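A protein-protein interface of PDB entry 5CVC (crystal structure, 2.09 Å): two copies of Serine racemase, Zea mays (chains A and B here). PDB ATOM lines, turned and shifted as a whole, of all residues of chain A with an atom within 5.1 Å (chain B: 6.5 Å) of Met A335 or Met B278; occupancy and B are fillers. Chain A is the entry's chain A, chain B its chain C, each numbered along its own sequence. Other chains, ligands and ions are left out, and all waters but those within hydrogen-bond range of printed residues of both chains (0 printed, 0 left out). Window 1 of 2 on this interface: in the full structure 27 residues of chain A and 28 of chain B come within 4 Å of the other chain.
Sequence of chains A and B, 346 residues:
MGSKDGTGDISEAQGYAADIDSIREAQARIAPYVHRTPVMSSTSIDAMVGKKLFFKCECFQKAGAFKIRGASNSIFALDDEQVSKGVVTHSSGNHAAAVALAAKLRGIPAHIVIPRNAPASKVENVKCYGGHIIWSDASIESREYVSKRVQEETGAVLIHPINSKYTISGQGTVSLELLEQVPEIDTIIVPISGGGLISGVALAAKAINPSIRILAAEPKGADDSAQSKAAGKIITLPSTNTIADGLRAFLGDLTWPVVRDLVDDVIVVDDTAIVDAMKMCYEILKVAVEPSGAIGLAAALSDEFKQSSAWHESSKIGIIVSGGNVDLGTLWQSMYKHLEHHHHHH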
ATOM      1  N   LEU A 331      10.818  10.575  16.112  1.00  0.00           N
ATOM      2  CA  LEU A 331      12.238  10.849  15.930  1.00  0.00           C
ATOM      3  C   LEU A 331      12.969  10.552  17.237  1.00  0.00           C
ATOM      4  O   LEU A 331      13.946   9.811  17.256  1.00  0.00           O
ATOM      5  CB  LEU A 331      12.471  12.319  15.550  1.00  0.00           C
ATOM      6  CG  LEU A 331      13.631  12.690  14.621  1.00  0.00           C
ATOM      7  CD1 LEU A 331      14.117  14.096  14.941  1.00  0.00           C
ATOM      8  CD2 LEU A 331      14.797  11.721  14.648  1.00  0.00           C
ATOM      9  N   TRP A 332      12.467  11.117  18.327  1.00  0.00           N
ATOM     10  CA  TRP A 332      13.157  11.030  19.616  1.00  0.00           C
ATOM     11  C   TRP A 332      13.216   9.623  20.157  1.00  0.00           C
ATOM     12  O   TRP A 332      14.251   9.211  20.667  1.00  0.00           O
ATOM     13  CB  TRP A 332      12.545  11.975  20.649  1.00  0.00           C
ATOM     14  CG  TRP A 332      12.397  13.347  20.105  1.00  0.00           C
ATOM     15  CD1 TRP A 332      11.282  14.129  20.160  1.00  0.00           C
ATOM     16  CD2 TRP A 332      13.377  14.091  19.375  1.00  0.00           C
ATOM     17  NE1 TRP A 332      11.514  15.323  19.535  1.00  0.00           N
ATOM     18  CE2 TRP A 332      12.792  15.325  19.038  1.00  0.00           C
ATOM     19  CE3 TRP A 332      14.704  13.844  18.988  1.00  0.00           C
ATOM     20  CZ2 TRP A 332      13.480  16.309  18.318  1.00  0.00           C
ATOM     21  CZ3 TRP A 332      15.383  14.822  18.282  1.00  0.00           C
ATOM     22  CH2 TRP A 332      14.767  16.039  17.954  1.00  0.00           C
ATOM     23  N   GLN A 333      12.121   8.889  20.013  1.00  0.00           N
ATOM     24  CA  GLN A 333      12.076   7.485  20.420  1.00  0.00           C
ATOM     25  C   GLN A 333      13.144   6.701  19.671  1.00  0.00           C
ATOM     26  O   GLN A 333      13.894   5.967  20.284  1.00  0.00           O
ATOM     27  CB  GLN A 333      10.695   6.867  20.167  1.00  0.00           C
ATOM     28  CG  GLN A 333       9.583   7.430  21.039  1.00  0.00           C
ATOM     29  N   SER A 334      13.239   6.890  18.356  1.00  0.00           N
ATOM     30  CA  SER A 334      14.272   6.205  17.572  1.00  0.00           C
ATOM     31  C   SER A 334      15.695   6.619  18.012  1.00  0.00           C
ATOM     32  O   SER A 334      16.602   5.782  18.092  1.00  0.00           O
ATOM     33  CB  SER A 334      14.066   6.417  16.062  1.00  0.00           C
ATOM     34  OG  SER A 334      14.682   7.609  15.596  1.00  0.00           O
ATOM     35  N   MET A 335      15.892   7.894  18.318  1.00  0.00           N
ATOM     36  CA  MET A 335      17.203   8.350  18.778  1.00  0.00           C
ATOM     37  C   MET A 335      17.605   7.763  20.126  1.00  0.00           C
ATOM     38  O   MET A 335      18.732   7.311  20.276  1.00  0.00           O
ATOM     39  CB  MET A 335      17.267   9.864  18.818  1.00  0.00           C
ATOM     40  CG  MET A 335      17.227  10.441  17.411  1.00  0.00           C
ATOM     41  SD  MET A 335      18.005  12.041  17.302  1.00  0.00           S
ATOM     42  CE  MET A 335      19.725  11.596  17.574  1.00  0.00           C
ATOM     43  N   TYR A 336      16.684   7.745  21.084  1.00  0.00           N
ATOM     44  CA  TYR A 336      16.960   7.134  22.388  1.00  0.00           C
ATOM     45  C   TYR A 336      17.276   5.640  22.229  1.00  0.00           C
ATOM     46  O   TYR A 336      18.161   5.131  22.905  1.00  0.00           O
ATOM     47  CB  TYR A 336      15.812   7.368  23.392  1.00  0.00           C
ATOM     48  CG  TYR A 336      15.692   8.810  23.879  1.00  0.00           C
ATOM     49  CD1 TYR A 336      16.737   9.420  24.565  1.00  0.00           C
ATOM     50  CD2 TYR A 336      14.522   9.563  23.653  1.00  0.00           C
ATOM     51  CE1 TYR A 336      16.637  10.735  25.008  1.00  0.00           C
ATOM     52  CE2 TYR A 336      14.412  10.877  24.094  1.00  0.00           C
ATOM     53  CZ  TYR A 336      15.471  11.462  24.773  1.00  0.00           C
ATOM     54  OH  TYR A 336      15.407  12.768  25.227  1.00  0.00           O
ATOM     55  N   LYS A 337      16.577   4.955  21.327  1.00  0.00           N
ATOM     56  CA  LYS A 337      16.871   3.541  21.020  1.00  0.00           C
ATOM     57  C   LYS A 337      18.275   3.383  20.448  1.00  0.00           C
ATOM     58  O   LYS A 337      19.034   2.514  20.863  1.00  0.00           O
ATOM     59  CB  LYS A 337      15.885   2.960  19.989  1.00  0.00           C
ATOM     60  CG  LYS A 337      14.655   2.268  20.553  1.00  0.00           C
ATOM     61  CD  LYS A 337      14.097   1.257  19.555  1.00  0.00           C
ATOM     62  N   HIS A 338      18.589   4.228  19.476  1.00  0.00           N
ATOM     63  CA  HIS A 338      19.839   4.145  18.724  1.00  0.00           C
ATOM     64  C   HIS A 338      21.049   4.375  19.612  1.00  0.00           C
ATOM     65  O   HIS A 338      22.041   3.666  19.488  1.00  0.00           O
ATOM     66  CB  HIS A 338      19.842   5.149  17.558  1.00  0.00           C
ATOM     67  CG  HIS A 338      18.862   4.823  16.467  1.00  0.00           C
ATOM     68  ND1 HIS A 338      17.963   3.775  16.544  1.00  0.00           N
ATOM     69  CD2 HIS A 338      18.609   5.444  15.287  1.00  0.00           C
ATOM     70  CE1 HIS A 338      17.221   3.749  15.450  1.00  0.00           C
ATOM     71  NE2 HIS A 338      17.594   4.749  14.670  1.00  0.00           N
ATOM     72  N   LEU A 339      20.979   5.347  20.514  1.00  0.00           N
ATOM     73  CA  LEU A 339      22.133   5.604  21.381  1.00  0.00           C
ATOM     74  C   LEU A 339      22.445   4.402  22.314  1.00  0.00           C
ATOM     75  O   LEU A 339      23.622   4.112  22.580  1.00  0.00           O
ATOM     76  CB  LEU A 339      21.988   6.917  22.159  1.00  0.00           C
ATOM     77  CG  LEU A 339      21.127   6.967  23.425  1.00  0.00           C
ATOM     78  CD1 LEU A 339      21.822   6.374  24.642  1.00  0.00           C
ATOM     79  CD2 LEU A 339      20.748   8.406  23.711  1.00  0.00           C
ATOM     80  N   ILE B 243      27.184   8.835  19.797  1.00  0.00           N
ATOM     81  CA  ILE B 243      26.354   9.169  18.643  1.00  0.00           C
ATOM     82  C   ILE B 243      26.700  10.558  18.058  1.00  0.00           C
ATOM     83  O   ILE B 243      26.302  10.882  16.955  1.00  0.00           O
ATOM     84  CB  ILE B 243      24.850   9.131  18.987  1.00  0.00           C
ATOM     85  CG1 ILE B 243      24.530  10.110  20.125  1.00  0.00           C
ATOM     86  CG2 ILE B 243      24.432   7.716  19.364  1.00  0.00           C
ATOM     87  CD1 ILE B 243      23.231  10.841  19.930  1.00  0.00           C
ATOM     88  N   ALA B 273      21.924  13.018  27.381  1.00  0.00           N
ATOM     89  CA  ALA B 273      21.843  14.440  27.602  1.00  0.00           C
ATOM     90  C   ALA B 273      21.967  15.199  26.261  1.00  0.00           C
ATOM     91  O   ALA B 273      21.311  16.223  26.053  1.00  0.00           O
ATOM     92  CB  ALA B 273      22.909  14.887  28.594  1.00  0.00           C
ATOM     93  N   ILE B 274      22.787  14.671  25.351  1.00  0.00           N
ATOM     94  CA  ILE B 274      22.936  15.248  24.009  1.00  0.00           C
ATOM     95  C   ILE B 274      21.618  15.178  23.222  1.00  0.00           C
ATOM     96  O   ILE B 274      21.172  16.180  22.638  1.00  0.00           O
ATOM     97  CB  ILE B 274      24.103  14.580  23.241  1.00  0.00           C
ATOM     98  CG1 ILE B 274      25.419  14.970  23.909  1.00  0.00           C
ATOM     99  CG2 ILE B 274      24.127  15.009  21.776  1.00  0.00           C
ATOM    100  CD1 ILE B 274      26.628  14.232  23.378  1.00  0.00           C
ATOM    101  N   VAL B 275      21.002  14.003  23.215  1.00  0.00           N
ATOM    102  CA  VAL B 275      19.683  13.837  22.608  1.00  0.00           C
ATOM    103  C   VAL B 275      18.641  14.739  23.290  1.00  0.00           C
ATOM    104  O   VAL B 275      17.883  15.422  22.603  1.00  0.00           O
ATOM    105  CB  VAL B 275      19.222  12.359  22.615  1.00  0.00           C
ATOM    106  CG1 VAL B 275      17.800  12.216  22.077  1.00  0.00           C
ATOM    107  CG2 VAL B 275      20.154  11.516  21.763  1.00  0.00           C
ATOM    108  N   ASP B 276      18.592  14.738  24.628  1.00  0.00           N
ATOM    109  CA  ASP B 276      17.699  15.660  25.353  1.00  0.00           C
ATOM    110  C   ASP B 276      17.903  17.106  24.872  1.00  0.00           C
ATOM    111  O   ASP B 276      16.944  17.851  24.692  1.00  0.00           O
ATOM    112  CB  ASP B 276      17.947  15.639  26.857  1.00  0.00           C
ATOM    113  CG  ASP B 276      17.579  14.325  27.524  1.00  0.00           C
ATOM    114  OD1 ASP B 276      16.859  13.487  26.941  1.00  0.00           O
ATOM    115  OD2 ASP B 276      18.026  14.147  28.677  1.00  0.00           O
ATOM    116  N   ALA B 277      19.159  17.516  24.696  1.00  0.00           N
ATOM    117  CA  ALA B 277      19.444  18.873  24.251  1.00  0.00           C
ATOM    118  C   ALA B 277      19.042  19.097  22.777  1.00  0.00           C
ATOM    119  O   ALA B 277      18.538  20.166  22.413  1.00  0.00           O
ATOM    120  CB  ALA B 277      20.908  19.218  24.474  1.00  0.00           C
ATOM    121  N   MET B 278      19.233  18.078  21.949  1.00  0.00           N
ATOM    122  CA  MET B 278      18.856  18.142  20.547  1.00  0.00           C
ATOM    123  C   MET B 278      17.345  18.357  20.408  1.00  0.00           C
ATOM    124  O   MET B 278      16.884  19.185  19.616  1.00  0.00           O
ATOM    125  CB  MET B 278      19.254  16.855  19.846  1.00  0.00           C
ATOM    126  CG  MET B 278      19.061  16.854  18.344  1.00  0.00           C
ATOM    127  SD  MET B 278      19.612  15.287  17.632  1.00  0.00           S
ATOM    128  CE  MET B 278      18.966  15.432  15.973  1.00  0.00           C
ATOM    129  N   LYS B 279      16.601  17.565  21.171  1.00  0.00           N
ATOM    130  CA  LYS B 279      15.161  17.680  21.276  1.00  0.00           C
ATOM    131  C   LYS B 279      14.705  19.108  21.619  1.00  0.00           C
ATOM    132  O   LYS B 279      13.781  19.622  21.008  1.00  0.00           O
ATOM    133  CB  LYS B 279      14.673  16.692  22.325  1.00  0.00           C
ATOM    134  CG  LYS B 279      13.178  16.694  22.589  1.00  0.00           C
ATOM    135  CD  LYS B 279      12.812  15.478  23.431  1.00  0.00           C
ATOM    136  CE  LYS B 279      11.313  15.260  23.505  1.00  0.00           C
ATOM    137  NZ  LYS B 279      10.661  16.352  24.266  1.00  0.00           N
ATOM    138  N   MET B 280      15.355  19.728  22.596  1.00  0.00           N
ATOM    139  CA  MET B 280      15.061  21.102  22.958  1.00  0.00           C
ATOM    140  C   MET B 280      15.345  22.079  21.823  1.00  0.00           C
ATOM    141  O   MET B 280      14.577  23.012  21.620  1.00  0.00           O
ATOM    142  CB  MET B 280      15.846  21.528  24.198  1.00  0.00           C
ATOM    143  CG  MET B 280      15.256  20.985  25.494  1.00  0.00           C
ATOM    144  SD  MET B 280      16.037  21.629  26.990  1.00  0.00           S
ATOM    145  CE  MET B 280      16.383  23.300  26.508  1.00  0.00           C
ATOM    146  N   CYS B 281      16.444  21.873  21.097  1.00  0.00           N
ATOM    147  CA  CYS B 281      16.789  22.735  19.947  1.00  0.00           C
ATOM    148  C   CYS B 281      15.702  22.681  18.884  1.00  0.00           C
ATOM    149  O   CYS B 281      15.325  23.706  18.339  1.00  0.00           O
ATOM    150  CB  CYS B 281      18.114  22.318  19.305  1.00  0.00           C
ATOM    151  SG  CYS B 281      19.574  22.740  20.275  1.00  0.00           S
ATOM    152  N   TYR B 282      15.220  21.481  18.588  1.00  0.00           N
ATOM    153  CA  TYR B 282      14.143  21.304  17.608  1.00  0.00           C
ATOM    154  C   TYR B 282      12.809  21.888  18.110  1.00  0.00           C
ATOM    155  O   TYR B 282      12.147  22.651  17.406  1.00  0.00           O
ATOM    156  CB  TYR B 282      13.954  19.815  17.260  1.00  0.00           C
ATOM    157  CG  TYR B 282      14.963  19.252  16.257  1.00  0.00           C
ATOM    158  CD1 TYR B 282      16.318  19.157  16.575  1.00  0.00           C
ATOM    159  CD2 TYR B 282      14.562  18.801  15.008  1.00  0.00           C
ATOM    160  CE1 TYR B 282      17.241  18.652  15.666  1.00  0.00           C
ATOM    161  CE2 TYR B 282      15.471  18.283  14.103  1.00  0.00           C
ATOM    162  CZ  TYR B 282      16.812  18.207  14.441  1.00  0.00           C
ATOM    163  OH  TYR B 282      17.724  17.693  13.547  1.00  0.00           O
ATOM    164  N   GLU B 283      12.447  21.551  19.341  1.00  0.00           N
ATOM    165  CA  GLU B 283      11.123  21.854  19.857  1.00  0.00           C
ATOM    166  C   GLU B 283      10.958  23.280  20.370  1.00  0.00           C
ATOM    167  O   GLU B 283       9.895  23.848  20.220  1.00  0.00           O
ATOM    168  CB  GLU B 283      10.753  20.858  20.959  1.00  0.00           C
ATOM    169  CG  GLU B 283      10.450  19.481  20.414  1.00  0.00           C
ATOM    170  CD  GLU B 283       9.916  18.531  21.478  1.00  0.00           C
ATOM    171  OE1 GLU B 283      10.167  18.755  22.680  1.00  0.00           O
ATOM    172  OE2 GLU B 283       9.241  17.562  21.103  1.00  0.00           O
ATOM    173  N   VAL B 287      15.300  24.828  15.634  1.00  0.00           N
ATOM    174  CA  VAL B 287      16.538  24.703  14.856  1.00  0.00           C
ATOM    175  C   VAL B 287      16.886  23.223  14.705  1.00  0.00           C
ATOM    176  O   VAL B 287      17.042  22.527  15.709  1.00  0.00           O
ATOM    177  CB  VAL B 287      17.686  25.457  15.540  1.00  0.00           C
ATOM    178  CG1 VAL B 287      18.963  25.368  14.720  1.00  0.00           C
ATOM    179  CG2 VAL B 287      17.299  26.915  15.738  1.00  0.00           C
ATOM    180  N   ALA B 288      16.997  22.761  13.463  1.00  0.00           N
ATOM    181  CA  ALA B 288      17.264  21.350  13.151  1.00  0.00           C
ATOM    182  C   ALA B 288      18.766  21.038  13.187  1.00  0.00           C
ATOM    183  O   ALA B 288      19.426  20.894  12.140  1.00  0.00           O
ATOM    184  CB  ALA B 288      16.676  20.963  11.789  1.00  0.00           C
ATOM    185  N   VAL B 289      19.280  20.962  14.405  1.00  0.00           N
ATOM    186  CA  VAL B 289      20.695  20.702  14.666  1.00  0.00           C
ATOM    187  C   VAL B 289      21.054  19.230  14.525  1.00  0.00           C
ATOM    188  O   VAL B 289      20.177  18.346  14.559  1.00  0.00           O
ATOM    189  CB  VAL B 289      21.103  21.153  16.093  1.00  0.00           C
ATOM    190  CG1 VAL B 289      20.869  22.643  16.280  1.00  0.00           C
ATOM    191  CG2 VAL B 289      20.352  20.376  17.159  1.00  0.00           C
ATOM    192  N   GLU B 290      22.356  18.960  14.404  1.00  0.00           N
ATOM    193  CA  GLU B 290      22.854  17.586  14.503  1.00  0.00           C
ATOM    194  C   GLU B 290      23.297  17.382  15.941  1.00  0.00           C
ATOM    195  O   GLU B 290      23.566  18.360  16.642  1.00  0.00           O
ATOM    196  CB  GLU B 290      24.013  17.322  13.515  1.00  0.00           C
ATOM    197  CG  GLU B 290      25.258  18.182  13.682  1.00  0.00           C
ATOM    198  CD  GLU B 290      26.318  17.845  12.637  1.00  0.00           C
ATOM    199  OE1 GLU B 290      26.901  16.761  12.762  1.00  0.00           O
ATOM    200  OE2 GLU B 290      26.541  18.630  11.683  1.00  0.00           O
ATOM    201  N   PRO B 291      23.383  16.122  16.395  1.00  0.00           N
ATOM    202  CA  PRO B 291      23.738  15.858  17.792  1.00  0.00           C
ATOM    203  C   PRO B 291      25.012  16.579  18.254  1.00  0.00           C
ATOM    204  O   PRO B 291      25.075  17.078  19.383  1.00  0.00           O
ATOM    205  CB  PRO B 291      23.956  14.338  17.818  1.00  0.00           C
ATOM    206  CG  PRO B 291      23.125  13.813  16.712  1.00  0.00           C
ATOM    207  CD  PRO B 291      23.139  14.874  15.646  1.00  0.00           C
ATOM    208  N   ALA B 294      24.410  20.087  19.363  1.00  0.00           N
ATOM    209  CA  ALA B 294      23.549  20.317  20.521  1.00  0.00           C
ATOM    210  C   ALA B 294      24.314  20.201  21.851  1.00  0.00           C
ATOM    211  O   ALA B 294      23.787  20.553  22.905  1.00  0.00           O
ATOM    212  CB  ALA B 294      22.391  19.341  20.510  1.00  0.00           C
ATOM    213  N   LEU B 297      24.578  22.907  24.601  1.00  0.00           N
ATOM    214  CA  LEU B 297      23.366  23.102  25.397  1.00  0.00           C
ATOM    215  C   LEU B 297      23.277  22.070  26.513  1.00  0.00           C
ATOM    216  O   LEU B 297      22.956  22.421  27.651  1.00  0.00           O
ATOM    217  CB  LEU B 297      22.114  23.053  24.517  1.00  0.00           C
ATOM    218  CG  LEU B 297      20.761  23.156  25.247  1.00  0.00           C
ATOM    219  CD1 LEU B 297      20.720  24.347  26.207  1.00  0.00           C
ATOM    220  CD2 LEU B 297      19.648  23.249  24.218  1.00  0.00           C
ATOM    221  N   VAL B 326      22.486  16.132   9.697  1.00  0.00           N
ATOM    222  CA  VAL B 326      22.055  14.914  10.381  1.00  0.00           C
ATOM    223  C   VAL B 326      21.047  14.179   9.514  1.00  0.00           C
ATOM    224  O   VAL B 326      20.207  14.796   8.887  1.00  0.00           O
ATOM    225  CB  VAL B 326      21.461  15.237  11.770  1.00  0.00           C
ATOM    226  CG1 VAL B 326      20.309  16.237  11.657  1.00  0.00           C
ATOM    227  CG2 VAL B 326      21.032  13.965  12.501  1.00  0.00           C
ATOM    228  N   LEU B 328      17.827  12.303   9.000  1.00  0.00           N
ATOM    229  CA  LEU B 328      16.541  12.148   9.669  1.00  0.00           C
ATOM    230  C   LEU B 328      15.613  11.232   8.859  1.00  0.00           C
ATOM    231  O   LEU B 328      14.386  11.328   8.966  1.00  0.00           O
ATOM    232  CB  LEU B 328      15.912  13.529   9.864  1.00  0.00           C
ATOM    233  CG  LEU B 328      16.837  14.504  10.603  1.00  0.00           C
ATOM    234  CD1 LEU B 328      16.426  15.949  10.370  1.00  0.00           C
ATOM    235  CD2 LEU B 328      16.878  14.179  12.088  1.00  0.00           C
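SD of Met A335 sits close to SD of Met B278 (3.6 Å). The side-chain hydroxyl of Tyr A336 sits close to the side-chain carboxylate of Asp B276 (2.4 Å).
O of Leu A331 lies within hydrogen-bond range of OG of Ser A334. The side-chain amino group (NZ) of Lys B279 is in salt-bridge range of the side-chain carboxylate (OE1) of Glu B283 (2.9 Å). OH of Tyr B282 lies within hydrogen-bond range of O of Val B289 (2.7 Å).
Among the printed residues, merely in contact across the chains: Leu A331 with Leu B328, Trp A332 with Lys B279, Trp A332 with Tyr B282, Trp A332 with Glu B283, Tyr A336 with Val B275, Leu A339 with Ile B243 and Leu A339 with Val B275.
Of chain B, only Met B278 comes within 4 Å of Met A335. Met B278 touches just one residue of chain A: Met A335. Printed residues of chain A within 4 Å of Tyr B282: Trp A332 (3.6 Å). Printed residues of chain A within 4 Å of Asp B276: Tyr A336 (2.4 Å). His A338 touches none of the printed residues of chain B. The nearest residue of chain B that does not touch Met A335 is Val B275 (4.1 Å). The nearest residue of chain A that does not touch Met B278 is Trp A332 (4.1 Å). The nearest printed residue of chain A that does not touch Asp B276 is Leu A339 (6.8 Å).
Of the 21 printed residues of chain B, 8 touch a printed residue of chain A. Hydrophobic or aromatic side chains of chain B that line the printed part of chain A: Ile B243, Val B275, Met B278, Tyr B282 and Leu B328.
No position is printed for both chains. Of the 9 pairs that touch across the chains among the printed residues, none has its exchanged pair printed and touching as well.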
